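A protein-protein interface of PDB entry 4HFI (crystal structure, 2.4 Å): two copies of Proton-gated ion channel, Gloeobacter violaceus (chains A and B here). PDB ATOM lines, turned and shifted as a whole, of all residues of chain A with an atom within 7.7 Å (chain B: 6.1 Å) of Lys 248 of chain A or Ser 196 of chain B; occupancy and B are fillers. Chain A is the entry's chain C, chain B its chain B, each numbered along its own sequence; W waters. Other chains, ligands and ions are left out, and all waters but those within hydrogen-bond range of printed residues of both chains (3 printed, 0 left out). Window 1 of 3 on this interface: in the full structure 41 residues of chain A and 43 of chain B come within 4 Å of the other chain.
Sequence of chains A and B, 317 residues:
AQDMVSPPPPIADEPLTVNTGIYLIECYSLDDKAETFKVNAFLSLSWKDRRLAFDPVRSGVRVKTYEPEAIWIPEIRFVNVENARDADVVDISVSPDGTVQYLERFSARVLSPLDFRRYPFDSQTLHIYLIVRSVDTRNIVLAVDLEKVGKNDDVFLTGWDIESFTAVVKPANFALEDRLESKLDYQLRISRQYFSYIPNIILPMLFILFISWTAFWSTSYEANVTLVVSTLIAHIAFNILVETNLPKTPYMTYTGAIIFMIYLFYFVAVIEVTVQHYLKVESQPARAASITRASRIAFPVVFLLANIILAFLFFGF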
ATOM      1  N   ASP A  32     -22.929  27.522  26.506  1.00  0.00           N
ATOM      2  CA  ASP A  32     -21.870  27.162  25.556  1.00  0.00           C
ATOM      3  C   ASP A  32     -22.323  26.155  24.506  1.00  0.00           C
ATOM      4  O   ASP A  32     -22.015  26.329  23.328  1.00  0.00           O
ATOM      5  CB  ASP A  32     -20.636  26.637  26.301  1.00  0.00           C
ATOM      6  CG  ASP A  32     -19.995  27.692  27.172  1.00  0.00           C
ATOM      7  OD1 ASP A  32     -19.378  28.623  26.618  1.00  0.00           O
ATOM      8  OD2 ASP A  32     -20.121  27.595  28.409  1.00  0.00           O
ATOM      9  N   LYS A  33     -23.056  25.111  24.927  1.00  0.00           N
ATOM     10  CA  LYS A  33     -23.577  24.062  24.047  1.00  0.00           C
ATOM     11  C   LYS A  33     -24.572  24.621  23.037  1.00  0.00           C
ATOM     12  O   LYS A  33     -24.459  24.321  21.845  1.00  0.00           O
ATOM     13  CB  LYS A  33     -24.215  22.928  24.866  1.00  0.00           C
ATOM     14  CG  LYS A  33     -23.376  21.669  24.904  1.00  0.00           C
ATOM     15  CD  LYS A  33     -23.988  20.614  25.815  1.00  0.00           C
ATOM     16  CE  LYS A  33     -23.876  19.211  25.262  1.00  0.00           C
ATOM     17  NZ  LYS A  33     -22.464  18.772  25.062  1.00  0.00           N
ATOM     18  N   GLU A  35     -24.915  27.898  22.352  1.00  0.00           N
ATOM     19  CA  GLU A  35     -24.308  29.119  21.796  1.00  0.00           C
ATOM     20  C   GLU A  35     -25.284  30.297  21.876  1.00  0.00           C
ATOM     21  O   GLU A  35     -25.459  31.066  20.927  1.00  0.00           O
ATOM     22  CB  GLU A  35     -23.688  28.891  20.403  1.00  0.00           C
ATOM     23  CG  GLU A  35     -22.399  28.091  20.481  1.00  0.00           C
ATOM     24  CD  GLU A  35     -21.776  27.702  19.157  1.00  0.00           C
ATOM     25  OE1 GLU A  35     -21.671  26.484  18.891  1.00  0.00           O
ATOM     26  OE2 GLU A  35     -21.358  28.605  18.399  1.00  0.00           O
ATOM     27  N   PHE A 116     -14.477  28.185  20.255  1.00  0.00           N
ATOM     28  CA  PHE A 116     -13.947  27.377  21.354  1.00  0.00           C
ATOM     29  C   PHE A 116     -12.484  26.947  21.209  1.00  0.00           C
ATOM     30  O   PHE A 116     -11.983  26.255  22.095  1.00  0.00           O
ATOM     31  CB  PHE A 116     -14.850  26.159  21.609  1.00  0.00           C
ATOM     32  CG  PHE A 116     -16.252  26.500  22.039  1.00  0.00           C
ATOM     33  CD1 PHE A 116     -16.543  26.765  23.371  1.00  0.00           C
ATOM     34  CD2 PHE A 116     -17.287  26.550  21.111  1.00  0.00           C
ATOM     35  CE1 PHE A 116     -17.844  27.076  23.769  1.00  0.00           C
ATOM     36  CE2 PHE A 116     -18.585  26.871  21.507  1.00  0.00           C
ATOM     37  CZ  PHE A 116     -18.860  27.119  22.835  1.00  0.00           C
ATOM     38  N   GLU A 243     -16.447  17.197  27.477  1.00  0.00           N
ATOM     39  CA  GLU A 243     -17.300  17.210  26.289  1.00  0.00           C
ATOM     40  C   GLU A 243     -18.796  17.457  26.551  1.00  0.00           C
ATOM     41  O   GLU A 243     -19.501  17.877  25.629  1.00  0.00           O
ATOM     42  CB  GLU A 243     -17.004  16.044  25.317  1.00  0.00           C
ATOM     43  CG  GLU A 243     -17.445  14.663  25.773  1.00  0.00           C
ATOM     44  CD  GLU A 243     -17.200  13.560  24.761  1.00  0.00           C
ATOM     45  OE1 GLU A 243     -16.189  12.836  24.904  1.00  0.00           O
ATOM     46  OE2 GLU A 243     -18.021  13.414  23.828  1.00  0.00           O
ATOM     47  N   LEU A 246     -19.376  21.244  26.419  1.00  0.00           N
ATOM     48  CA  LEU A 246     -19.055  21.818  25.115  1.00  0.00           C
ATOM     49  C   LEU A 246     -19.881  21.282  23.955  1.00  0.00           C
ATOM     50  O   LEU A 246     -20.164  20.080  23.921  1.00  0.00           O
ATOM     51  CB  LEU A 246     -17.576  21.531  24.787  1.00  0.00           C
ATOM     52  CG  LEU A 246     -16.507  22.247  25.590  1.00  0.00           C
ATOM     53  CD1 LEU A 246     -15.151  21.665  25.288  1.00  0.00           C
ATOM     54  CD2 LEU A 246     -16.502  23.728  25.291  1.00  0.00           C
ATOM     55  N   PRO A 247     -20.161  22.107  22.918  1.00  0.00           N
ATOM     56  CA  PRO A 247     -20.817  21.554  21.727  1.00  0.00           C
ATOM     57  C   PRO A 247     -19.775  20.829  20.860  1.00  0.00           C
ATOM     58  O   PRO A 247     -18.567  20.970  21.076  1.00  0.00           O
ATOM     59  CB  PRO A 247     -21.349  22.799  21.017  1.00  0.00           C
ATOM     60  CG  PRO A 247     -20.414  23.872  21.393  1.00  0.00           C
ATOM     61  CD  PRO A 247     -19.860  23.547  22.747  1.00  0.00           C
ATOM     62  N   LYS A 248     -20.238  20.077  19.866  1.00  0.00           N
ATOM     63  CA  LYS A 248     -19.352  19.383  18.942  1.00  0.00           C
ATOM     64  C   LYS A 248     -18.823  20.409  17.934  1.00  0.00           C
ATOM     65  O   LYS A 248     -19.613  21.142  17.328  1.00  0.00           O
ATOM     66  CB  LYS A 248     -20.092  18.210  18.286  1.00  0.00           C
ATOM     67  CG  LYS A 248     -20.191  17.024  19.238  1.00  0.00           C
ATOM     68  CD  LYS A 248     -21.431  16.187  19.038  1.00  0.00           C
ATOM     69  CE  LYS A 248     -21.524  15.143  20.124  1.00  0.00           C
ATOM     70  NZ  LYS A 248     -22.668  14.217  19.908  1.00  0.00           N
ATOM     71  N   THR A 249     -17.488  20.521  17.823  1.00  0.00           N
ATOM     72  CA  THR A 249     -16.832  21.508  16.955  1.00  0.00           C
ATOM     73  C   THR A 249     -16.142  20.891  15.727  1.00  0.00           C
ATOM     74  O   THR A 249     -15.532  19.827  15.850  1.00  0.00           O
ATOM     75  CB  THR A 249     -15.860  22.390  17.764  1.00  0.00           C
ATOM     76  OG1 THR A 249     -14.913  21.561  18.441  1.00  0.00           O
ATOM     77  CG2 THR A 249     -16.572  23.290  18.763  1.00  0.00           C
ATOM     78  N   PRO A 250     -16.162  21.554  14.542  1.00  0.00           N
ATOM     79  CA  PRO A 250     -15.448  20.981  13.384  1.00  0.00           C
ATOM     80  C   PRO A 250     -13.942  21.291  13.418  1.00  0.00           C
ATOM     81  O   PRO A 250     -13.270  21.261  12.385  1.00  0.00           O
ATOM     82  CB  PRO A 250     -16.162  21.612  12.185  1.00  0.00           C
ATOM     83  CG  PRO A 250     -16.687  22.919  12.694  1.00  0.00           C
ATOM     84  CD  PRO A 250     -16.802  22.844  14.196  1.00  0.00           C
ATOM     85  N   TYR A 251     -13.418  21.592  14.614  1.00  0.00           N
ATOM     86  CA  TYR A 251     -12.021  21.922  14.880  1.00  0.00           C
ATOM     87  C   TYR A 251     -11.629  21.411  16.263  1.00  0.00           C
ATOM     88  O   TYR A 251     -12.508  21.079  17.070  1.00  0.00           O
ATOM     89  CB  TYR A 251     -11.793  23.451  14.795  1.00  0.00           C
ATOM     90  CG  TYR A 251     -12.706  24.279  15.679  1.00  0.00           C
ATOM     91  CD1 TYR A 251     -13.829  24.914  15.153  1.00  0.00           C
ATOM     92  CD2 TYR A 251     -12.438  24.444  17.036  1.00  0.00           C
ATOM     93  CE1 TYR A 251     -14.677  25.670  15.962  1.00  0.00           C
ATOM     94  CE2 TYR A 251     -13.283  25.191  17.855  1.00  0.00           C
ATOM     95  CZ  TYR A 251     -14.398  25.808  17.313  1.00  0.00           C
ATOM     96  OH  TYR A 251     -15.227  26.552  18.121  1.00  0.00           O
ATOM     97  N   MET A 252     -10.315  21.370  16.545  1.00  0.00           N
ATOM     98  CA  MET A 252      -9.807  20.961  17.848  1.00  0.00           C
ATOM     99  C   MET A 252      -9.770  22.163  18.777  1.00  0.00           C
ATOM    100  O   MET A 252      -9.347  23.247  18.368  1.00  0.00           O
ATOM    101  CB  MET A 252      -8.379  20.375  17.747  1.00  0.00           C
ATOM    102  CG  MET A 252      -8.280  19.006  17.105  1.00  0.00           C
ATOM    103  SD  MET A 252      -9.217  17.687  17.921  1.00  0.00           S
ATOM    104  CE  MET A 252      -8.151  17.307  19.296  1.00  0.00           C
ATOM    105  N   THR A 253     -10.204  21.972  20.027  1.00  0.00           N
ATOM    106  CA  THR A 253     -10.116  23.004  21.058  1.00  0.00           C
ATOM    107  C   THR A 253      -8.781  22.753  21.779  1.00  0.00           C
ATOM    108  O   THR A 253      -8.228  21.651  21.666  1.00  0.00           O
ATOM    109  CB  THR A 253     -11.323  22.964  22.014  1.00  0.00           C
ATOM    110  OG1 THR A 253     -11.275  21.784  22.809  1.00  0.00           O
ATOM    111  CG2 THR A 253     -12.660  23.071  21.294  1.00  0.00           C
ATOM    112  N   TYR B 119     -24.661   7.328  10.765  1.00  0.00           N
ATOM    113  CA  TYR B 119     -24.179   8.134  11.894  1.00  0.00           C
ATOM    114  C   TYR B 119     -22.761   7.724  12.367  1.00  0.00           C
ATOM    115  O   TYR B 119     -22.501   6.524  12.498  1.00  0.00           O
ATOM    116  CB  TYR B 119     -25.194   8.055  13.049  1.00  0.00           C
ATOM    117  CG  TYR B 119     -24.843   8.850  14.286  1.00  0.00           C
ATOM    118  CD1 TYR B 119     -24.135   8.270  15.336  1.00  0.00           C
ATOM    119  CD2 TYR B 119     -25.284  10.160  14.443  1.00  0.00           C
ATOM    120  CE1 TYR B 119     -23.834   8.989  16.490  1.00  0.00           C
ATOM    121  CE2 TYR B 119     -24.991  10.887  15.595  1.00  0.00           C
ATOM    122  CZ  TYR B 119     -24.267  10.297  16.617  1.00  0.00           C
ATOM    123  OH  TYR B 119     -24.000  11.016  17.756  1.00  0.00           O
ATOM    124  N   THR B 158     -25.282  24.408  14.467  1.00  0.00           N
ATOM    125  CA  THR B 158     -24.221  23.824  15.300  1.00  0.00           C
ATOM    126  C   THR B 158     -24.102  22.309  15.105  1.00  0.00           C
ATOM    127  O   THR B 158     -25.091  21.587  15.257  1.00  0.00           O
ATOM    128  CB  THR B 158     -24.390  24.251  16.770  1.00  0.00           C
ATOM    129  OG1 THR B 158     -24.472  25.679  16.832  1.00  0.00           O
ATOM    130  CG2 THR B 158     -23.257  23.758  17.667  1.00  0.00           C
ATOM    131  N   GLY B 159     -22.909  21.877  14.706  1.00  0.00           N
ATOM    132  CA  GLY B 159     -22.585  20.479  14.436  1.00  0.00           C
ATOM    133  C   GLY B 159     -22.976  19.985  13.054  1.00  0.00           C
ATOM    134  O   GLY B 159     -22.844  18.793  12.771  1.00  0.00           O
ATOM    135  N   GLN B 193     -21.211  17.238  10.733  1.00  0.00           N
ATOM    136  CA  GLN B 193     -19.800  17.517  10.967  1.00  0.00           C
ATOM    137  C   GLN B 193     -19.328  16.418  11.914  1.00  0.00           C
ATOM    138  O   GLN B 193     -19.525  16.500  13.133  1.00  0.00           O
ATOM    139  CB  GLN B 193     -19.593  18.920  11.571  1.00  0.00           C
ATOM    140  CG  GLN B 193     -19.960  20.055  10.617  1.00  0.00           C
ATOM    141  CD  GLN B 193     -19.786  21.429  11.217  1.00  0.00           C
ATOM    142  OE1 GLN B 193     -19.839  21.629  12.435  1.00  0.00           O
ATOM    143  NE2 GLN B 193     -19.616  22.417  10.358  1.00  0.00           N
ATOM    144  N   TYR B 194     -18.778  15.348  11.325  1.00  0.00           N
ATOM    145  CA  TYR B 194     -18.283  14.157  12.018  1.00  0.00           C
ATOM    146  C   TYR B 194     -16.958  14.363  12.763  1.00  0.00           C
ATOM    147  O   TYR B 194     -16.603  13.513  13.585  1.00  0.00           O
ATOM    148  CB  TYR B 194     -18.145  12.987  11.026  1.00  0.00           C
ATOM    149  CG  TYR B 194     -17.257  13.291   9.837  1.00  0.00           C
ATOM    150  CD1 TYR B 194     -15.874  13.172   9.926  1.00  0.00           C
ATOM    151  CD2 TYR B 194     -17.803  13.666   8.612  1.00  0.00           C
ATOM    152  CE1 TYR B 194     -15.052  13.458   8.839  1.00  0.00           C
ATOM    153  CE2 TYR B 194     -16.991  13.945   7.516  1.00  0.00           C
ATOM    154  CZ  TYR B 194     -15.616  13.841   7.635  1.00  0.00           C
ATOM    155  OH  TYR B 194     -14.809  14.117   6.559  1.00  0.00           O
ATOM    156  N   PHE B 195     -16.211  15.449  12.443  1.00  0.00           N
ATOM    157  CA  PHE B 195     -14.894  15.783  13.004  1.00  0.00           C
ATOM    158  C   PHE B 195     -14.663  15.357  14.453  1.00  0.00           C
ATOM    159  O   PHE B 195     -13.810  14.509  14.696  1.00  0.00           O
ATOM    160  CB  PHE B 195     -14.540  17.280  12.811  1.00  0.00           C
ATOM    161  CG  PHE B 195     -13.160  17.670  13.308  1.00  0.00           C
ATOM    162  CD1 PHE B 195     -12.924  17.901  14.661  1.00  0.00           C
ATOM    163  CD2 PHE B 195     -12.101  17.822  12.422  1.00  0.00           C
ATOM    164  CE1 PHE B 195     -11.646  18.222  15.124  1.00  0.00           C
ATOM    165  CE2 PHE B 195     -10.826  18.172  12.883  1.00  0.00           C
ATOM    166  CZ  PHE B 195     -10.609  18.374  14.232  1.00  0.00           C
ATOM    167  N   SER B 196     -15.397  15.969  15.403  1.00  0.00           N
ATOM    168  CA  SER B 196     -15.251  15.756  16.850  1.00  0.00           C
ATOM    169  C   SER B 196     -15.434  14.320  17.333  1.00  0.00           C
ATOM    170  O   SER B 196     -14.891  13.972  18.381  1.00  0.00           O
ATOM    171  CB  SER B 196     -16.156  16.705  17.630  1.00  0.00           C
ATOM    172  OG  SER B 196     -17.508  16.455  17.288  1.00  0.00           O
ATOM    173  N   TYR B 197     -16.186  13.486  16.584  1.00  0.00           N
ATOM    174  CA  TYR B 197     -16.421  12.080  16.928  1.00  0.00           C
ATOM    175  C   TYR B 197     -15.137  11.255  16.869  1.00  0.00           C
ATOM    176  O   TYR B 197     -15.016  10.275  17.604  1.00  0.00           O
ATOM    177  CB  TYR B 197     -17.508  11.464  16.028  1.00  0.00           C
ATOM    178  CG  TYR B 197     -18.878  12.060  16.261  1.00  0.00           C
ATOM    179  CD1 TYR B 197     -19.757  11.495  17.177  1.00  0.00           C
ATOM    180  CD2 TYR B 197     -19.291  13.200  15.574  1.00  0.00           C
ATOM    181  CE1 TYR B 197     -21.016  12.047  17.406  1.00  0.00           C
ATOM    182  CE2 TYR B 197     -20.546  13.764  15.798  1.00  0.00           C
ATOM    183  CZ  TYR B 197     -21.409  13.181  16.713  1.00  0.00           C
ATOM    184  OH  TYR B 197     -22.655  13.721  16.937  1.00  0.00           O
ATOM    185  N   ILE B 198     -14.182  11.667  16.014  1.00  0.00           N
ATOM    186  CA  ILE B 198     -12.882  11.008  15.848  1.00  0.00           C
ATOM    187  C   ILE B 198     -12.019  11.130  17.136  1.00  0.00           C
ATOM    188  O   ILE B 198     -11.746  10.081  17.726  1.00  0.00           O
ATOM    189  CB  ILE B 198     -12.152  11.436  14.534  1.00  0.00           C
ATOM    190  CG1 ILE B 198     -13.067  11.258  13.291  1.00  0.00           C
ATOM    191  CG2 ILE B 198     -10.823  10.688  14.362  1.00  0.00           C
ATOM    192  CD1 ILE B 198     -12.688  12.110  12.083  1.00  0.00           C
ATOM    193  N   PRO B 199     -11.620  12.336  17.639  1.00  0.00           N
ATOM    194  CA  PRO B 199     -10.804  12.369  18.866  1.00  0.00           C
ATOM    195  C   PRO B 199     -11.565  12.080  20.166  1.00  0.00           C
ATOM    196  O   PRO B 199     -10.929  11.739  21.160  1.00  0.00           O
ATOM    197  CB  PRO B 199     -10.230  13.788  18.865  1.00  0.00           C
ATOM    198  CG  PRO B 199     -11.249  14.591  18.171  1.00  0.00           C
ATOM    199  CD  PRO B 199     -11.820  13.702  17.108  1.00  0.00           C
ATOM    200  N   ASN B 200     -12.903  12.248  20.177  1.00  0.00           N
ATOM    201  CA  ASN B 200     -13.704  12.061  21.394  1.00  0.00           C
ATOM    202  C   ASN B 200     -14.284  10.680  21.634  1.00  0.00           C
ATOM    203  O   ASN B 200     -14.376  10.269  22.793  1.00  0.00           O
ATOM    204  CB  ASN B 200     -14.786  13.125  21.521  1.00  0.00           C
ATOM    205  CG  ASN B 200     -14.234  14.500  21.770  1.00  0.00           C
ATOM    206  OD1 ASN B 200     -13.652  14.786  22.827  1.00  0.00           O
ATOM    207  ND2 ASN B 200     -14.415  15.387  20.804  1.00  0.00           N
ATOM    208  N   ILE B 201     -14.715   9.981  20.566  1.00  0.00           N
ATOM    209  CA  ILE B 201     -15.325   8.655  20.678  1.00  0.00           C
ATOM    210  C   ILE B 201     -14.555   7.553  19.939  1.00  0.00           C
ATOM    211  O   ILE B 201     -14.136   6.596  20.582  1.00  0.00           O
ATOM    212  CB  ILE B 201     -16.860   8.684  20.365  1.00  0.00           C
ATOM    213  CG1 ILE B 201     -17.631   9.416  21.486  1.00  0.00           C
ATOM    214  CG2 ILE B 201     -17.439   7.269  20.183  1.00  0.00           C
ATOM    215  CD1 ILE B 201     -18.545  10.459  21.035  1.00  0.00           C
ATOM    216  N   ASN B 245     -26.907  10.244  22.985  1.00  0.00           N
ATOM    217  CA  ASN B 245     -26.974  11.266  21.934  1.00  0.00           C
ATOM    218  C   ASN B 245     -27.899  10.825  20.788  1.00  0.00           C
ATOM    219  O   ASN B 245     -28.134  11.605  19.869  1.00  0.00           O
ATOM    220  CB  ASN B 245     -25.561  11.556  21.360  1.00  0.00           C
ATOM    221  CG  ASN B 245     -24.428  11.759  22.355  1.00  0.00           C
ATOM    222  OD1 ASN B 245     -24.622  12.174  23.506  1.00  0.00           O
ATOM    223  ND2 ASN B 245     -23.202  11.493  21.914  1.00  0.00           N
HETATM  224  O   HOH W   1     -19.116  20.034  14.774  1.00  0.00           O
HETATM  225  O   HOH W   2     -14.799  10.690  25.427  1.00  0.00           O
HETATM  226  O   HOH W   3     -17.788  17.490  14.806  1.00  0.00           O
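The side-chain hydroxyl of Tyr 197 of chain B is in hydrogen-bond range of the side-chain amino group of Lys 248 of chain A, 3.0 Å away. The side-chain amino group of Lys 248 of chain A lies close to the side-chain amide nitrogen of Asn 245 of chain B, 3.4 Å away.
The side-chain hydroxyl (OH) of Tyr 197 of chain B sits at hydrogen-bond distance from the side-chain hydroxyl (OH) of Tyr 119 of chain B (3.1 Å). O of Gly 159 of chain B sits at hydrogen-bond distance from N of Gln 193 of chain B, at 3.0 Å. ND2 of Asn 200 of chain B sits at hydrogen-bond distance from O of Ser 196 of chain B. NZ of Lys 33 of chain A is in hydrogen-bond range of O of Glu 243 of chain A, at 3.1 Å. The backbone NH of Phe 116 of chain A is in hydrogen-bond range of the side-chain hydroxyl of Tyr 251 of chain A (2.8 Å). O of Tyr 251 of chain A lies within hydrogen-bond range of OG1 of Thr 249 of chain A.
Among the printed residues, merely in contact across the chains: Lys 248 of chain A with Ser 196 of chain B (3.3 Å), Glu 35 of chain A with Thr 158 of chain B (3.4 Å), Tyr 251 of chain A with Phe 195 of chain B (3.4 Å), Pro 250 of chain A with Gln 193 of chain B (3.4 Å), Thr 249 of chain A with Phe 195 of chain B (3.5 Å), Pro 250 of chain A with Phe 195 of chain B (3.6 Å), Thr 249 of chain A with Ser 196 of chain B (3.6 Å), Glu 243 of chain A with Asn 200 of chain B (3.7 Å), Met 252 of chain A with Phe 195 of chain B (3.7 Å), Met 252 of chain A with Pro 199 of chain B (3.7 Å) and Pro 247 of chain A with Thr 158 of chain B (3.97 Å).
Of the printed residues of chain B, Lys 248 of chain A touches Ser 196 (3.3 Å), Tyr 197 (3.0 Å) and Asn 245 (3.4 Å). Of chain A, only Lys 248 (3.3 Å) and Thr 249 (3.6 Å) come within 4 Å of Ser 196 of chain B. Printed residues of chain B within 4 Å of Tyr 251 of chain A: Phe 195. Printed residues of chain A within 4 Å of Asn 245 of chain B: Lys 248. Tyr 194 of chain B touches none of the printed residues of chain A. The nearest residue of chain B that does not touch Lys 248 of chain A is Tyr 119 of chain B (4.1 Å). The nearest residue of chain A that does not touch Ser 196 of chain B is Pro 250 of chain A (5.4 Å).
Of the 13 printed residues of chain A, 8 touch a printed residue of chain B. Hydrophobic or aromatic side chains of chain A within 4 Å of the printed part of chain B: Pro 247, Pro 250 and Met 252. Among the printed residues, 13 pairs touch across the chains. Among the printed residues, no Asp or Glu carboxylate lies within 4 Å of a Lys or Arg side-chain nitrogen of the other chain.
No position is printed for both chains. Of the 13 pairs that touch across the chains among the printed residues, none has its exchanged pair printed and touching as well.
Water W3 lies within hydrogen-bond range of O of Gln 193 of chain B, OG of Ser 196 of chain B, O of Thr 249 of chain A and N of Phe 195 of chain B. Water W2 bridges the side-chain carboxylate of Glu 243 of chain A and the backbone carbonyl oxygen of Asn 200 of chain B. Water W1 lies within hydrogen-bond range of the backbone carbonyl oxygen of Lys 248 of chain A (2.8 Å), the side-chain amide oxygen of Gln 193 of chain B (2.9 Å) and the backbone NH of Thr 249 of chain A (3.5 Å).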
